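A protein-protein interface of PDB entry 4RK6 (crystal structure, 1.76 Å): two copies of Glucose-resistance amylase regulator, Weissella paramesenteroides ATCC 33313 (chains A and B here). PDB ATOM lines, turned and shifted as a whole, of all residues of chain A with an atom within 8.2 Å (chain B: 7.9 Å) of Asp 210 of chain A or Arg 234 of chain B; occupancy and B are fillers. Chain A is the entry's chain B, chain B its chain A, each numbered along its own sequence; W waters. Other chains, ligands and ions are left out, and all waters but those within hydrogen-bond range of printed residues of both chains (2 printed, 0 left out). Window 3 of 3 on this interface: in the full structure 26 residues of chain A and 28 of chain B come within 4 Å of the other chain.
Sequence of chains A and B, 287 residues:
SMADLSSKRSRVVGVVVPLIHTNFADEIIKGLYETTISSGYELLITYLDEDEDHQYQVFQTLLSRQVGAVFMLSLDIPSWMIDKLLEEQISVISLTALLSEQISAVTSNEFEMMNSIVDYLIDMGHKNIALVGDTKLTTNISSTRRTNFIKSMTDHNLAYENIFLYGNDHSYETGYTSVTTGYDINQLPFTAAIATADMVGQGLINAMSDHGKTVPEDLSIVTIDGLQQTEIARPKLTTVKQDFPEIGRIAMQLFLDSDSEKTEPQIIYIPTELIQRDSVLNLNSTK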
ATOM      1  N   TYR A 172       9.349 -20.111  -1.787  1.00  0.00           N
ATOM      2  CA  TYR A 172      10.612 -19.472  -2.034  1.00  0.00           C
ATOM      3  C   TYR A 172      10.726 -18.937  -3.450  1.00  0.00           C
ATOM      4  O   TYR A 172      11.156 -17.811  -3.674  1.00  0.00           O
ATOM      5  CB  TYR A 172      11.727 -20.489  -1.785  1.00  0.00           C
ATOM      6  CG  TYR A 172      13.112 -20.004  -2.107  1.00  0.00           C
ATOM      7  CD1 TYR A 172      13.895 -19.350  -1.153  1.00  0.00           C
ATOM      8  CD2 TYR A 172      13.689 -20.269  -3.357  1.00  0.00           C
ATOM      9  CE1 TYR A 172      15.187 -18.932  -1.453  1.00  0.00           C
ATOM     10  CE2 TYR A 172      14.971 -19.859  -3.651  1.00  0.00           C
ATOM     11  CZ  TYR A 172      15.715 -19.180  -2.708  1.00  0.00           C
ATOM     12  OH  TYR A 172      16.987 -18.812  -3.013  1.00  0.00           O
ATOM     13  N   TYR A 176      11.634 -15.215  -4.947  1.00  0.00           N
ATOM     14  CA  TYR A 176      12.777 -15.047  -5.808  1.00  0.00           C
ATOM     15  C   TYR A 176      12.364 -14.416  -7.136  1.00  0.00           C
ATOM     16  O   TYR A 176      13.036 -13.498  -7.597  1.00  0.00           O
ATOM     17  CB  TYR A 176      13.518 -16.383  -6.025  1.00  0.00           C
ATOM     18  CG  TYR A 176      14.958 -16.181  -6.434  1.00  0.00           C
ATOM     19  CD1 TYR A 176      15.285 -15.839  -7.737  1.00  0.00           C
ATOM     20  CD2 TYR A 176      16.001 -16.299  -5.514  1.00  0.00           C
ATOM     21  CE1 TYR A 176      16.602 -15.612  -8.115  1.00  0.00           C
ATOM     22  CE2 TYR A 176      17.324 -16.086  -5.888  1.00  0.00           C
ATOM     23  CZ  TYR A 176      17.617 -15.742  -7.194  1.00  0.00           C
ATOM     24  OH  TYR A 176      18.928 -15.528  -7.556  1.00  0.00           O
ATOM     25  N   THR A 180      12.885 -10.629 -10.060  1.00  0.00           N
ATOM     26  CA  THR A 180      13.710 -11.011 -11.208  1.00  0.00           C
ATOM     27  C   THR A 180      12.905 -11.008 -12.513  1.00  0.00           C
ATOM     28  O   THR A 180      13.288 -10.347 -13.475  1.00  0.00           O
ATOM     29  CB  THR A 180      14.437 -12.340 -10.965  1.00  0.00           C
ATOM     30  OG1 THR A 180      13.497 -13.354 -10.657  1.00  0.00           O
ATOM     31  CG2 THR A 180      15.397 -12.207  -9.796  1.00  0.00           C
ATOM     32  N   ILE A 185      14.779  -5.322 -10.801  1.00  0.00           N
ATOM     33  CA  ILE A 185      15.534  -5.301  -9.547  1.00  0.00           C
ATOM     34  C   ILE A 185      16.393  -4.048  -9.374  1.00  0.00           C
ATOM     35  O   ILE A 185      16.722  -3.648  -8.258  1.00  0.00           O
ATOM     36  CB  ILE A 185      16.382  -6.592  -9.420  1.00  0.00           C
ATOM     37  CG1 ILE A 185      16.751  -6.866  -7.966  1.00  0.00           C
ATOM     38  CG2 ILE A 185      17.601  -6.550 -10.336  1.00  0.00           C
ATOM     39  CD1 ILE A 185      17.208  -8.296  -7.751  1.00  0.00           C
ATOM     40  N   GLN A 202      12.692 -15.305   2.365  1.00  0.00           N
ATOM     41  CA  GLN A 202      14.013 -15.821   2.071  1.00  0.00           C
ATOM     42  C   GLN A 202      14.343 -15.759   0.578  1.00  0.00           C
ATOM     43  O   GLN A 202      15.490 -15.450   0.201  1.00  0.00           O
ATOM     44  CB  GLN A 202      14.193 -17.248   2.601  1.00  0.00           C
ATOM     45  CG  GLN A 202      15.647 -17.716   2.532  1.00  0.00           C
ATOM     46  CD  GLN A 202      16.566 -16.831   3.373  1.00  0.00           C
ATOM     47  OE1 GLN A 202      16.322 -16.652   4.555  1.00  0.00           O
ATOM     48  NE2 GLN A 202      17.607 -16.286   2.780  1.00  0.00           N
ATOM     49  N   GLY A 203      13.346 -16.031  -0.261  1.00  0.00           N
ATOM     50  CA  GLY A 203      13.494 -15.864  -1.704  1.00  0.00           C
ATOM     51  C   GLY A 203      13.836 -14.450  -2.088  1.00  0.00           C
ATOM     52  O   GLY A 203      14.746 -14.223  -2.898  1.00  0.00           O
ATOM     53  N   LEU A 204      13.143 -13.485  -1.482  1.00  0.00           N
ATOM     54  CA  LEU A 204      13.468 -12.066  -1.700  1.00  0.00           C
ATOM     55  C   LEU A 204      14.910 -11.747  -1.277  1.00  0.00           C
ATOM     56  O   LEU A 204      15.654 -11.124  -2.037  1.00  0.00           O
ATOM     57  CB  LEU A 204      12.479 -11.138  -0.971  1.00  0.00           C
ATOM     58  CG  LEU A 204      11.077 -11.099  -1.596  1.00  0.00           C
ATOM     59  CD1 LEU A 204      10.013 -10.657  -0.600  1.00  0.00           C
ATOM     60  CD2 LEU A 204      11.080 -10.230  -2.842  1.00  0.00           C
ATOM     61  N   ILE A 205      15.299 -12.159  -0.062  1.00  0.00           N
ATOM     62  CA  ILE A 205      16.655 -11.909   0.437  1.00  0.00           C
ATOM     63  C   ILE A 205      17.685 -12.448  -0.546  1.00  0.00           C
ATOM     64  O   ILE A 205      18.633 -11.758  -0.929  1.00  0.00           O
ATOM     65  CB  ILE A 205      16.889 -12.525   1.836  1.00  0.00           C
ATOM     66  CG1 ILE A 205      16.193 -11.664   2.899  1.00  0.00           C
ATOM     67  CG2 ILE A 205      18.379 -12.595   2.137  1.00  0.00           C
ATOM     68  CD1 ILE A 205      16.242 -12.250   4.288  1.00  0.00           C
ATOM     69  N   ASN A 206      17.507 -13.691  -0.957  1.00  0.00           N
ATOM     70  CA  ASN A 206      18.489 -14.316  -1.835  1.00  0.00           C
ATOM     71  C   ASN A 206      18.521 -13.696  -3.225  1.00  0.00           C
ATOM     72  O   ASN A 206      19.589 -13.549  -3.808  1.00  0.00           O
ATOM     73  CB  ASN A 206      18.248 -15.821  -1.913  1.00  0.00           C
ATOM     74  CG  ASN A 206      18.765 -16.552  -0.699  1.00  0.00           C
ATOM     75  OD1 ASN A 206      19.313 -15.950   0.230  1.00  0.00           O
ATOM     76  ND2 ASN A 206      18.629 -17.842  -0.709  1.00  0.00           N
ATOM     77  N   ALA A 207      17.365 -13.316  -3.765  1.00  0.00           N
ATOM     78  CA  ALA A 207      17.369 -12.672  -5.091  1.00  0.00           C
ATOM     79  C   ALA A 207      18.103 -11.356  -5.013  1.00  0.00           C
ATOM     80  O   ALA A 207      18.893 -11.032  -5.895  1.00  0.00           O
ATOM     81  CB  ALA A 207      15.953 -12.439  -5.605  1.00  0.00           C
ATOM     82  N   MET A 208      17.852 -10.580  -3.960  1.00  0.00           N
ATOM     83  CA  MET A 208      18.559  -9.297  -3.791  1.00  0.00           C
ATOM     84  C   MET A 208      20.048  -9.539  -3.659  1.00  0.00           C
ATOM     85  O   MET A 208      20.845  -8.942  -4.392  1.00  0.00           O
ATOM     86  CB  MET A 208      18.021  -8.502  -2.589  1.00  0.00           C
ATOM     87  CG  MET A 208      16.537  -8.133  -2.632  1.00  0.00           C
ATOM     88  SD  MET A 208      16.091  -7.080  -4.254  1.00  0.00           S
ATOM     89  CE  MET A 208      16.807  -5.342  -3.698  1.00  0.00           C
ATOM     90  N   SER A 209      20.448 -10.437  -2.774  1.00  0.00           N
ATOM     91  CA  SER A 209      21.861 -10.704  -2.555  1.00  0.00           C
ATOM     92  C   SER A 209      22.555 -11.272  -3.790  1.00  0.00           C
ATOM     93  O   SER A 209      23.676 -10.871  -4.118  1.00  0.00           O
ATOM     94  CB  SER A 209      22.063 -11.653  -1.370  1.00  0.00           C
ATOM     95  OG  SER A 209      23.419 -11.650  -0.978  1.00  0.00           O
ATOM     96  N   ASP A 210      21.893 -12.191  -4.482  1.00  0.00           N
ATOM     97  CA  ASP A 210      22.481 -12.784  -5.664  1.00  0.00           C
ATOM     98  C   ASP A 210      22.742 -11.763  -6.777  1.00  0.00           C
ATOM     99  O   ASP A 210      23.565 -12.012  -7.647  1.00  0.00           O
ATOM    100  CB  ASP A 210      21.603 -13.902  -6.233  1.00  0.00           C
ATOM    101  CG  ASP A 210      21.562 -15.155  -5.336  1.00  0.00           C
ATOM    102  OD1 ASP A 210      22.354 -15.264  -4.379  1.00  0.00           O
ATOM    103  OD2 ASP A 210      20.691 -16.014  -5.586  1.00  0.00           O
ATOM    104  N   HIS A 211      22.027 -10.645  -6.761  1.00  0.00           N
ATOM    105  CA  HIS A 211      22.173  -9.598  -7.794  1.00  0.00           C
ATOM    106  C   HIS A 211      22.938  -8.376  -7.263  1.00  0.00           C
ATOM    107  O   HIS A 211      22.839  -7.286  -7.820  1.00  0.00           O
ATOM    108  CB  HIS A 211      20.796  -9.208  -8.336  1.00  0.00           C
ATOM    109  CG  HIS A 211      20.145 -10.288  -9.136  1.00  0.00           C
ATOM    110  ND1 HIS A 211      19.483 -11.354  -8.555  1.00  0.00           N
ATOM    111  CD2 HIS A 211      20.091 -10.493 -10.474  1.00  0.00           C
ATOM    112  CE1 HIS A 211      19.036 -12.157  -9.504  1.00  0.00           C
ATOM    113  NE2 HIS A 211      19.390 -11.658 -10.676  1.00  0.00           N
ATOM    114  N   GLY A 212      23.694  -8.576  -6.185  1.00  0.00           N
ATOM    115  CA  GLY A 212      24.598  -7.564  -5.636  1.00  0.00           C
ATOM    116  C   GLY A 212      23.928  -6.483  -4.799  1.00  0.00           C
ATOM    117  O   GLY A 212      24.544  -5.451  -4.524  1.00  0.00           O
ATOM    118  N   LYS A 213      22.671  -6.710  -4.408  1.00  0.00           N
ATOM    119  CA  LYS A 213      21.918  -5.764  -3.581  1.00  0.00           C
ATOM    120  C   LYS A 213      21.961  -6.219  -2.132  1.00  0.00           C
ATOM    121  O   LYS A 213      22.436  -7.319  -1.826  1.00  0.00           O
ATOM    122  CB  LYS A 213      20.454  -5.645  -4.037  1.00  0.00           C
ATOM    123  CG  LYS A 213      20.223  -5.537  -5.544  1.00  0.00           C
ATOM    124  CD  LYS A 213      20.548  -4.173  -6.097  1.00  0.00           C
ATOM    125  CE  LYS A 213      20.404  -4.173  -7.608  1.00  0.00           C
ATOM    126  NZ  LYS A 213      21.059  -2.987  -8.217  1.00  0.00           N
ATOM    127  N   THR A 214      21.468  -5.375  -1.239  1.00  0.00           N
ATOM    128  CA  THR A 214      21.493  -5.666   0.197  1.00  0.00           C
ATOM    129  C   THR A 214      20.147  -5.321   0.829  1.00  0.00           C
ATOM    130  O   THR A 214      19.609  -4.256   0.573  1.00  0.00           O
ATOM    131  CB  THR A 214      22.593  -4.845   0.896  1.00  0.00           C
ATOM    132  OG1 THR A 214      23.871  -5.179   0.331  1.00  0.00           O
ATOM    133  CG2 THR A 214      22.624  -5.123   2.387  1.00  0.00           C
ATOM    134  N   ILE A 232      17.092 -17.745  10.856  1.00  0.00           N
ATOM    135  CA  ILE A 232      18.231 -18.263  10.103  1.00  0.00           C
ATOM    136  C   ILE A 232      18.647 -17.323   8.969  1.00  0.00           C
ATOM    137  O   ILE A 232      19.802 -17.306   8.546  1.00  0.00           O
ATOM    138  CB  ILE A 232      17.865 -19.651   9.543  1.00  0.00           C
ATOM    139  CG1 ILE A 232      17.718 -20.627  10.711  1.00  0.00           C
ATOM    140  CG2 ILE A 232      18.871 -20.124   8.502  1.00  0.00           C
ATOM    141  CD1 ILE A 232      17.007 -21.895  10.286  1.00  0.00           C
ATOM    142  N   ARG A 234      19.773 -14.041   6.980  1.00  0.00           N
ATOM    143  CA  ARG A 234      20.681 -12.938   7.227  1.00  0.00           C
ATOM    144  C   ARG A 234      20.459 -11.918   6.113  1.00  0.00           C
ATOM    145  O   ARG A 234      20.724 -12.226   4.936  1.00  0.00           O
ATOM    146  CB  ARG A 234      22.139 -13.408   7.288  1.00  0.00           C
ATOM    147  CG  ARG A 234      22.447 -14.337   8.457  1.00  0.00           C
ATOM    148  CD  ARG A 234      22.453 -13.576   9.778  1.00  0.00           C
ATOM    149  NE  ARG A 234      22.833 -14.398  10.922  1.00  0.00           N
ATOM    150  CZ  ARG A 234      22.012 -15.204  11.597  1.00  0.00           C
ATOM    151  NH1 ARG A 234      20.742 -15.373  11.219  1.00  0.00           N
ATOM    152  NH2 ARG A 234      22.468 -15.892  12.627  1.00  0.00           N
ATOM    153  N   GLN B 202      23.773 -25.225   7.770  1.00  0.00           N
ATOM    154  CA  GLN B 202      23.283 -23.858   7.823  1.00  0.00           C
ATOM    155  C   GLN B 202      23.770 -23.139   9.108  1.00  0.00           C
ATOM    156  O   GLN B 202      24.081 -21.933   9.094  1.00  0.00           O
ATOM    157  CB  GLN B 202      21.773 -23.852   7.717  1.00  0.00           C
ATOM    158  CG  GLN B 202      21.146 -22.489   7.777  1.00  0.00           C
ATOM    159  CD  GLN B 202      21.419 -21.677   6.535  1.00  0.00           C
ATOM    160  OE1 GLN B 202      20.728 -21.839   5.512  1.00  0.00           O
ATOM    161  NE2 GLN B 202      22.417 -20.800   6.603  1.00  0.00           N
ATOM    162  N   ILE B 205      27.397 -22.157   8.631  1.00  0.00           N
ATOM    163  CA  ILE B 205      27.509 -20.986   7.767  1.00  0.00           C
ATOM    164  C   ILE B 205      27.227 -19.706   8.558  1.00  0.00           C
ATOM    165  O   ILE B 205      27.991 -18.726   8.488  1.00  0.00           O
ATOM    166  CB  ILE B 205      26.542 -21.082   6.576  1.00  0.00           C
ATOM    167  CG1 ILE B 205      27.074 -22.082   5.549  1.00  0.00           C
ATOM    168  CG2 ILE B 205      26.326 -19.702   5.951  1.00  0.00           C
ATOM    169  CD1 ILE B 205      26.097 -22.317   4.417  1.00  0.00           C
ATOM    170  N   ASN B 206      26.144 -19.715   9.320  1.00  0.00           N
ATOM    171  CA  ASN B 206      25.767 -18.521  10.062  1.00  0.00           C
ATOM    172  C   ASN B 206      26.750 -18.189  11.171  1.00  0.00           C
ATOM    173  O   ASN B 206      26.997 -17.010  11.414  1.00  0.00           O
ATOM    174  CB  ASN B 206      24.329 -18.615  10.593  1.00  0.00           C
ATOM    175  CG  ASN B 206      23.309 -18.335   9.515  1.00  0.00           C
ATOM    176  OD1 ASN B 206      23.670 -18.004   8.395  1.00  0.00           O
ATOM    177  ND2 ASN B 206      22.046 -18.450   9.840  1.00  0.00           N
ATOM    178  N   SER B 209      29.663 -16.508   9.456  1.00  0.00           N
ATOM    179  CA  SER B 209      29.279 -15.155   8.973  1.00  0.00           C
ATOM    180  C   SER B 209      29.117 -14.154  10.103  1.00  0.00           C
ATOM    181  O   SER B 209      29.497 -12.994   9.955  1.00  0.00           O
ATOM    182  CB  SER B 209      27.958 -15.184   8.185  1.00  0.00           C
ATOM    183  OG  SER B 209      28.082 -15.972   7.032  1.00  0.00           O
ATOM    184  N   THR B 214      33.894 -16.314   6.460  1.00  0.00           N
ATOM    185  CA  THR B 214      33.095 -16.696   5.320  1.00  0.00           C
ATOM    186  C   THR B 214      33.380 -18.133   4.935  1.00  0.00           C
ATOM    187  O   THR B 214      34.529 -18.553   4.932  1.00  0.00           O
ATOM    188  CB  THR B 214      33.427 -15.790   4.115  1.00  0.00           C
ATOM    189  OG1 THR B 214      33.296 -14.415   4.517  1.00  0.00           O
ATOM    190  CG2 THR B 214      32.491 -16.064   2.943  1.00  0.00           C
ATOM    191  N   VAL B 215      32.316 -18.864   4.616  1.00  0.00           N
ATOM    192  CA  VAL B 215      32.414 -20.204   4.025  1.00  0.00           C
ATOM    193  C   VAL B 215      32.420 -20.007   2.523  1.00  0.00           C
ATOM    194  O   VAL B 215      31.573 -19.254   2.027  1.00  0.00           O
ATOM    195  CB  VAL B 215      31.170 -21.031   4.434  1.00  0.00           C
ATOM    196  CG1 VAL B 215      31.100 -22.351   3.686  1.00  0.00           C
ATOM    197  CG2 VAL B 215      31.151 -21.273   5.936  1.00  0.00           C
ATOM    198  N   PRO B 216      33.320 -20.642   1.772  1.00  0.00           N
ATOM    199  CA  PRO B 216      34.260 -21.695   2.229  1.00  0.00           C
ATOM    200  C   PRO B 216      35.678 -21.231   2.598  1.00  0.00           C
ATOM    201  O   PRO B 216      36.475 -22.049   3.046  1.00  0.00           O
ATOM    202  CB  PRO B 216      34.352 -22.609   1.014  1.00  0.00           C
ATOM    203  CG  PRO B 216      34.166 -21.682  -0.140  1.00  0.00           C
ATOM    204  CD  PRO B 216      33.125 -20.680   0.310  1.00  0.00           C
ATOM    205  N   GLN B 228      16.019 -28.900   0.721  1.00  0.00           N
ATOM    206  CA  GLN B 228      15.926 -27.512   0.266  1.00  0.00           C
ATOM    207  C   GLN B 228      16.873 -26.527   0.956  1.00  0.00           C
ATOM    208  O   GLN B 228      17.356 -25.604   0.324  1.00  0.00           O
ATOM    209  CB  GLN B 228      14.488 -27.002   0.412  1.00  0.00           C
ATOM    210  CG  GLN B 228      14.292 -25.582  -0.092  1.00  0.00           C
ATOM    211  CD  GLN B 228      12.894 -25.051   0.157  1.00  0.00           C
ATOM    212  OE1 GLN B 228      12.279 -25.327   1.193  1.00  0.00           O
ATOM    213  NE2 GLN B 228      12.393 -24.259  -0.784  1.00  0.00           N
ATOM    214  N   GLN B 229      17.145 -26.713   2.236  1.00  0.00           N
ATOM    215  CA  GLN B 229      18.082 -25.798   2.924  1.00  0.00           C
ATOM    216  C   GLN B 229      19.430 -25.660   2.219  1.00  0.00           C
ATOM    217  O   GLN B 229      20.050 -24.573   2.244  1.00  0.00           O
ATOM    218  CB  GLN B 229      18.266 -26.195   4.388  1.00  0.00           C
ATOM    219  CG  GLN B 229      18.660 -25.055   5.285  1.00  0.00           C
ATOM    220  CD  GLN B 229      17.520 -24.051   5.485  1.00  0.00           C
ATOM    221  OE1 GLN B 229      16.340 -24.424   5.546  1.00  0.00           O
ATOM    222  NE2 GLN B 229      17.864 -22.797   5.591  1.00  0.00           N
ATOM    223  N   THR B 230      19.899 -26.726   1.562  1.00  0.00           N
ATOM    224  CA  THR B 230      21.180 -26.661   0.855  1.00  0.00           C
ATOM    225  C   THR B 230      21.171 -25.737  -0.357  1.00  0.00           C
ATOM    226  O   THR B 230      22.200 -25.217  -0.745  1.00  0.00           O
ATOM    227  CB  THR B 230      21.689 -28.053   0.419  1.00  0.00           C
ATOM    228  OG1 THR B 230      20.832 -28.611  -0.594  1.00  0.00           O
ATOM    229  CG2 THR B 230      21.784 -28.973   1.601  1.00  0.00           C
ATOM    230  N   GLU B 231      19.984 -25.521  -0.920  1.00  0.00           N
ATOM    231  CA  GLU B 231      19.771 -24.633  -2.071  1.00  0.00           C
ATOM    232  C   GLU B 231      19.504 -23.178  -1.670  1.00  0.00           C
ATOM    233  O   GLU B 231      19.759 -22.261  -2.457  1.00  0.00           O
ATOM    234  CB  GLU B 231      18.568 -25.135  -2.881  1.00  0.00           C
ATOM    235  CG  GLU B 231      18.644 -26.584  -3.356  1.00  0.00           C
ATOM    236  CD  GLU B 231      17.274 -27.190  -3.657  1.00  0.00           C
ATOM    237  OE1 GLU B 231      16.276 -26.445  -3.796  1.00  0.00           O
ATOM    238  OE2 GLU B 231      17.187 -28.432  -3.745  1.00  0.00           O
ATOM    239  N   ILE B 232      18.964 -22.972  -0.477  1.00  0.00           N
ATOM    240  CA  ILE B 232      18.643 -21.601  -0.026  1.00  0.00           C
ATOM    241  C   ILE B 232      19.762 -21.005   0.827  1.00  0.00           C
ATOM    242  O   ILE B 232      19.820 -19.796   1.011  1.00  0.00           O
ATOM    243  CB  ILE B 232      17.253 -21.473   0.654  1.00  0.00           C
ATOM    244  CG1 ILE B 232      17.210 -22.102   2.019  1.00  0.00           C
ATOM    245  CG2 ILE B 232      16.160 -22.080  -0.206  1.00  0.00           C
ATOM    246  CD1 ILE B 232      15.829 -22.063   2.655  1.00  0.00           C
ATOM    247  N   ALA B 233      20.668 -21.850   1.315  1.00  0.00           N
ATOM    248  CA  ALA B 233      21.870 -21.383   2.006  1.00  0.00           C
ATOM    249  C   ALA B 233      22.712 -20.552   1.058  1.00  0.00           C
ATOM    250  O   ALA B 233      22.669 -20.743  -0.175  1.00  0.00           O
ATOM    251  CB  ALA B 233      22.701 -22.566   2.494  1.00  0.00           C
ATOM    252  N   ARG B 234      23.482 -19.639   1.629  1.00  0.00           N
ATOM    253  CA  ARG B 234      24.453 -18.858   0.874  1.00  0.00           C
ATOM    254  C   ARG B 234      25.741 -18.815   1.662  1.00  0.00           C
ATOM    255  O   ARG B 234      25.787 -18.198   2.726  1.00  0.00           O
ATOM    256  CB  ARG B 234      23.931 -17.443   0.578  1.00  0.00           C
ATOM    257  CG  ARG B 234      22.762 -17.401  -0.400  1.00  0.00           C
ATOM    258  CD  ARG B 234      23.199 -17.675  -1.840  1.00  0.00           C
ATOM    259  NE  ARG B 234      22.107 -17.595  -2.811  1.00  0.00           N
ATOM    260  CZ  ARG B 234      21.182 -18.534  -3.040  1.00  0.00           C
ATOM    261  NH1 ARG B 234      21.129 -19.662  -2.329  1.00  0.00           N
ATOM    262  NH2 ARG B 234      20.263 -18.324  -3.981  1.00  0.00           N
ATOM    263  N   PRO B 235      26.789 -19.483   1.181  1.00  0.00           N
ATOM    264  CA  PRO B 235      26.841 -20.180  -0.113  1.00  0.00           C
ATOM    265  C   PRO B 235      25.990 -21.435  -0.171  1.00  0.00           C
ATOM    266  O   PRO B 235      25.749 -22.088   0.867  1.00  0.00           O
ATOM    267  CB  PRO B 235      28.314 -20.601  -0.197  1.00  0.00           C
ATOM    268  CG  PRO B 235      28.702 -20.832   1.233  1.00  0.00           C
ATOM    269  CD  PRO B 235      28.006 -19.721   1.975  1.00  0.00           C
ATOM    270  N   LYS B 236      25.546 -21.805  -1.375  1.00  0.00           N
ATOM    271  CA  LYS B 236      24.818 -23.063  -1.544  1.00  0.00           C
ATOM    272  C   LYS B 236      25.710 -24.212  -1.071  1.00  0.00           C
ATOM    273  O   LYS B 236      26.922 -24.221  -1.325  1.00  0.00           O
ATOM    274  CB  LYS B 236      24.405 -23.270  -3.004  1.00  0.00           C
ATOM    275  CG  LYS B 236      23.316 -22.314  -3.497  1.00  0.00           C
ATOM    276  CD  LYS B 236      23.103 -22.446  -5.001  1.00  0.00           C
ATOM    277  CE  LYS B 236      21.889 -21.661  -5.493  1.00  0.00           C
ATOM    278  NZ  LYS B 236      20.588 -22.373  -5.307  1.00  0.00           N
ATOM    279  N   LEU B 237      25.099 -25.176  -0.405  1.00  0.00           N
ATOM    280  CA  LEU B 237      25.849 -26.254   0.245  1.00  0.00           C
ATOM    281  C   LEU B 237      26.057 -27.456  -0.645  1.00  0.00           C
ATOM    282  O   LEU B 237      25.112 -28.022  -1.203  1.00  0.00           O
ATOM    283  CB  LEU B 237      25.147 -26.684   1.538  1.00  0.00           C
ATOM    284  CG  LEU B 237      25.290 -25.706   2.688  1.00  0.00           C
ATOM    285  CD1 LEU B 237      24.140 -25.872   3.676  1.00  0.00           C
ATOM    286  CD2 LEU B 237      26.654 -25.884   3.377  1.00  0.00           C
ATOM    287  N   ASP B 278      28.799 -24.701  -3.646  1.00  0.00           N
ATOM    288  CA  ASP B 278      29.678 -23.547  -3.422  1.00  0.00           C
ATOM    289  C   ASP B 278      30.362 -23.491  -2.055  1.00  0.00           C
ATOM    290  O   ASP B 278      30.984 -22.494  -1.710  1.00  0.00           O
ATOM    291  CB  ASP B 278      28.878 -22.257  -3.666  1.00  0.00           C
ATOM    292  CG  ASP B 278      28.397 -22.141  -5.098  1.00  0.00           C
ATOM    293  OD1 ASP B 278      29.162 -22.485  -6.014  1.00  0.00           O
ATOM    294  OD2 ASP B 278      27.259 -21.711  -5.316  1.00  0.00           O
ATOM    295  N   SER B 279      30.312 -24.577  -1.300  1.00  0.00           N
ATOM    296  CA  SER B 279      30.780 -24.544   0.081  1.00  0.00           C
ATOM    297  C   SER B 279      32.073 -25.300   0.353  1.00  0.00           C
ATOM    298  O   SER B 279      32.401 -25.526   1.517  1.00  0.00           O
ATOM    299  CB  SER B 279      29.672 -25.045   1.028  1.00  0.00           C
ATOM    300  OG  SER B 279      29.377 -26.410   0.816  1.00  0.00           O
HETATM  301  O   HOH W   1       9.399 -23.015  -0.755  1.00  0.00           O
HETATM  302  O   HOH W   2      18.236 -20.099  -4.938  1.00  0.00           O
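The side-chain amide nitrogen of Asn 206 of chain B is in hydrogen-bond range of the backbone carbonyl oxygen of Ile 232 of chain A (2.8 Å). The side-chain amide nitrogen (ND2) of Asn 206 of chain A is in hydrogen-bond range of the backbone carbonyl oxygen (O) of Ile 232 of chain B, at 2.9 Å. OH of Tyr 172 of chain A lies within hydrogen-bond range of NH2 of Arg 234 of chain B, at 3.5 Å. The guanidinium group (NH1) of Arg 234 of chain B sits close to the side-chain amide nitrogen (ND2) of Asn 206 of chain A. NE of Arg 234 of chain B is in salt-bridge range of OD1 of Asp 210 of chain A.
The backbone carbonyl oxygen of Glu 231 of chain B sits at hydrogen-bond distance from the guanidinium group of Arg 234 of chain B, at 2.9 Å. The side-chain hydroxyl (OH) of Tyr 176 of chain A sits at hydrogen-bond distance from the side-chain carboxylate (OD2) of Asp 210 of chain A, 2.7 Å away.
Among the printed residues, merely in contact across the chains: Ile 232 of chain A with Gln 202 of chain B (3.4 Å), Tyr 172 of chain A with Ile 232 of chain B (3.5 Å), Arg 234 of chain A with Asn 206 of chain B (3.6 Å) and Tyr 172 of chain A with Gln 228 of chain B (3.96 Å).
Asp 210 of chain A touches one residue of chain B. No residue of chain A comes within 4 Å of Ala 233 of chain B. No residue of chain A comes within 4 Å of Pro 235 of chain B. Of the printed residues of chain A, Gln 202 of chain B touches Ile 232. Printed residues of chain B within 4 Å of Ile 232 of chain A: Gln 202 and Asn 206. Of the printed residues of chain B, Tyr 172 of chain A touches Gln 228 (3.96 Å), Ile 232 (3.5 Å) and Arg 234 (3.5 Å). The nearest printed residue of chain B that does not touch Asp 210 of chain A is Lys 236 of chain B (5.8 Å). The nearest residue of chain A that does not touch Arg 234 of chain B is Tyr 176 of chain A (4.2 Å). The nearest printed residue of chain A that does not touch Asn 206 of chain B is Gln 202 of chain A (8.0 Å).
Printed residues of chain B that touch a printed residue of chain A: Gln 202, Asn 206, Gln 228, Ile 232 and Arg 234. Of the 19 printed residues of chain A, 5 touch a printed residue of chain B. Among the printed residues, 9 pairs touch across the chains. Among the printed residues, Asp or Glu carboxylates within 4 Å of a Lys or Arg side-chain nitrogen of the other chain: Asp 210 of chain A with Arg 234 of chain B (2.8 Å).
Asn 206 of chain A touches Ile 232 of chain B, and with the chains exchanged Ile 232 of chain A touches Asn 206 of chain B. Asn 206 of chain A touches Arg 234 of chain B, and with the chains exchanged Arg 234 of chain A touches Asn 206 of chain B. Positions printed for both chains: 202, 205, 206, 209, 214, 232 and 234.
Water W2 lies within hydrogen-bond range of the side-chain hydroxyl of Tyr 172 of chain A (2.6 Å), the guanidinium group of Arg 234 of chain B (2.9 Å) and the side-chain amino group of Lys 236 of chain B (3.3 Å).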
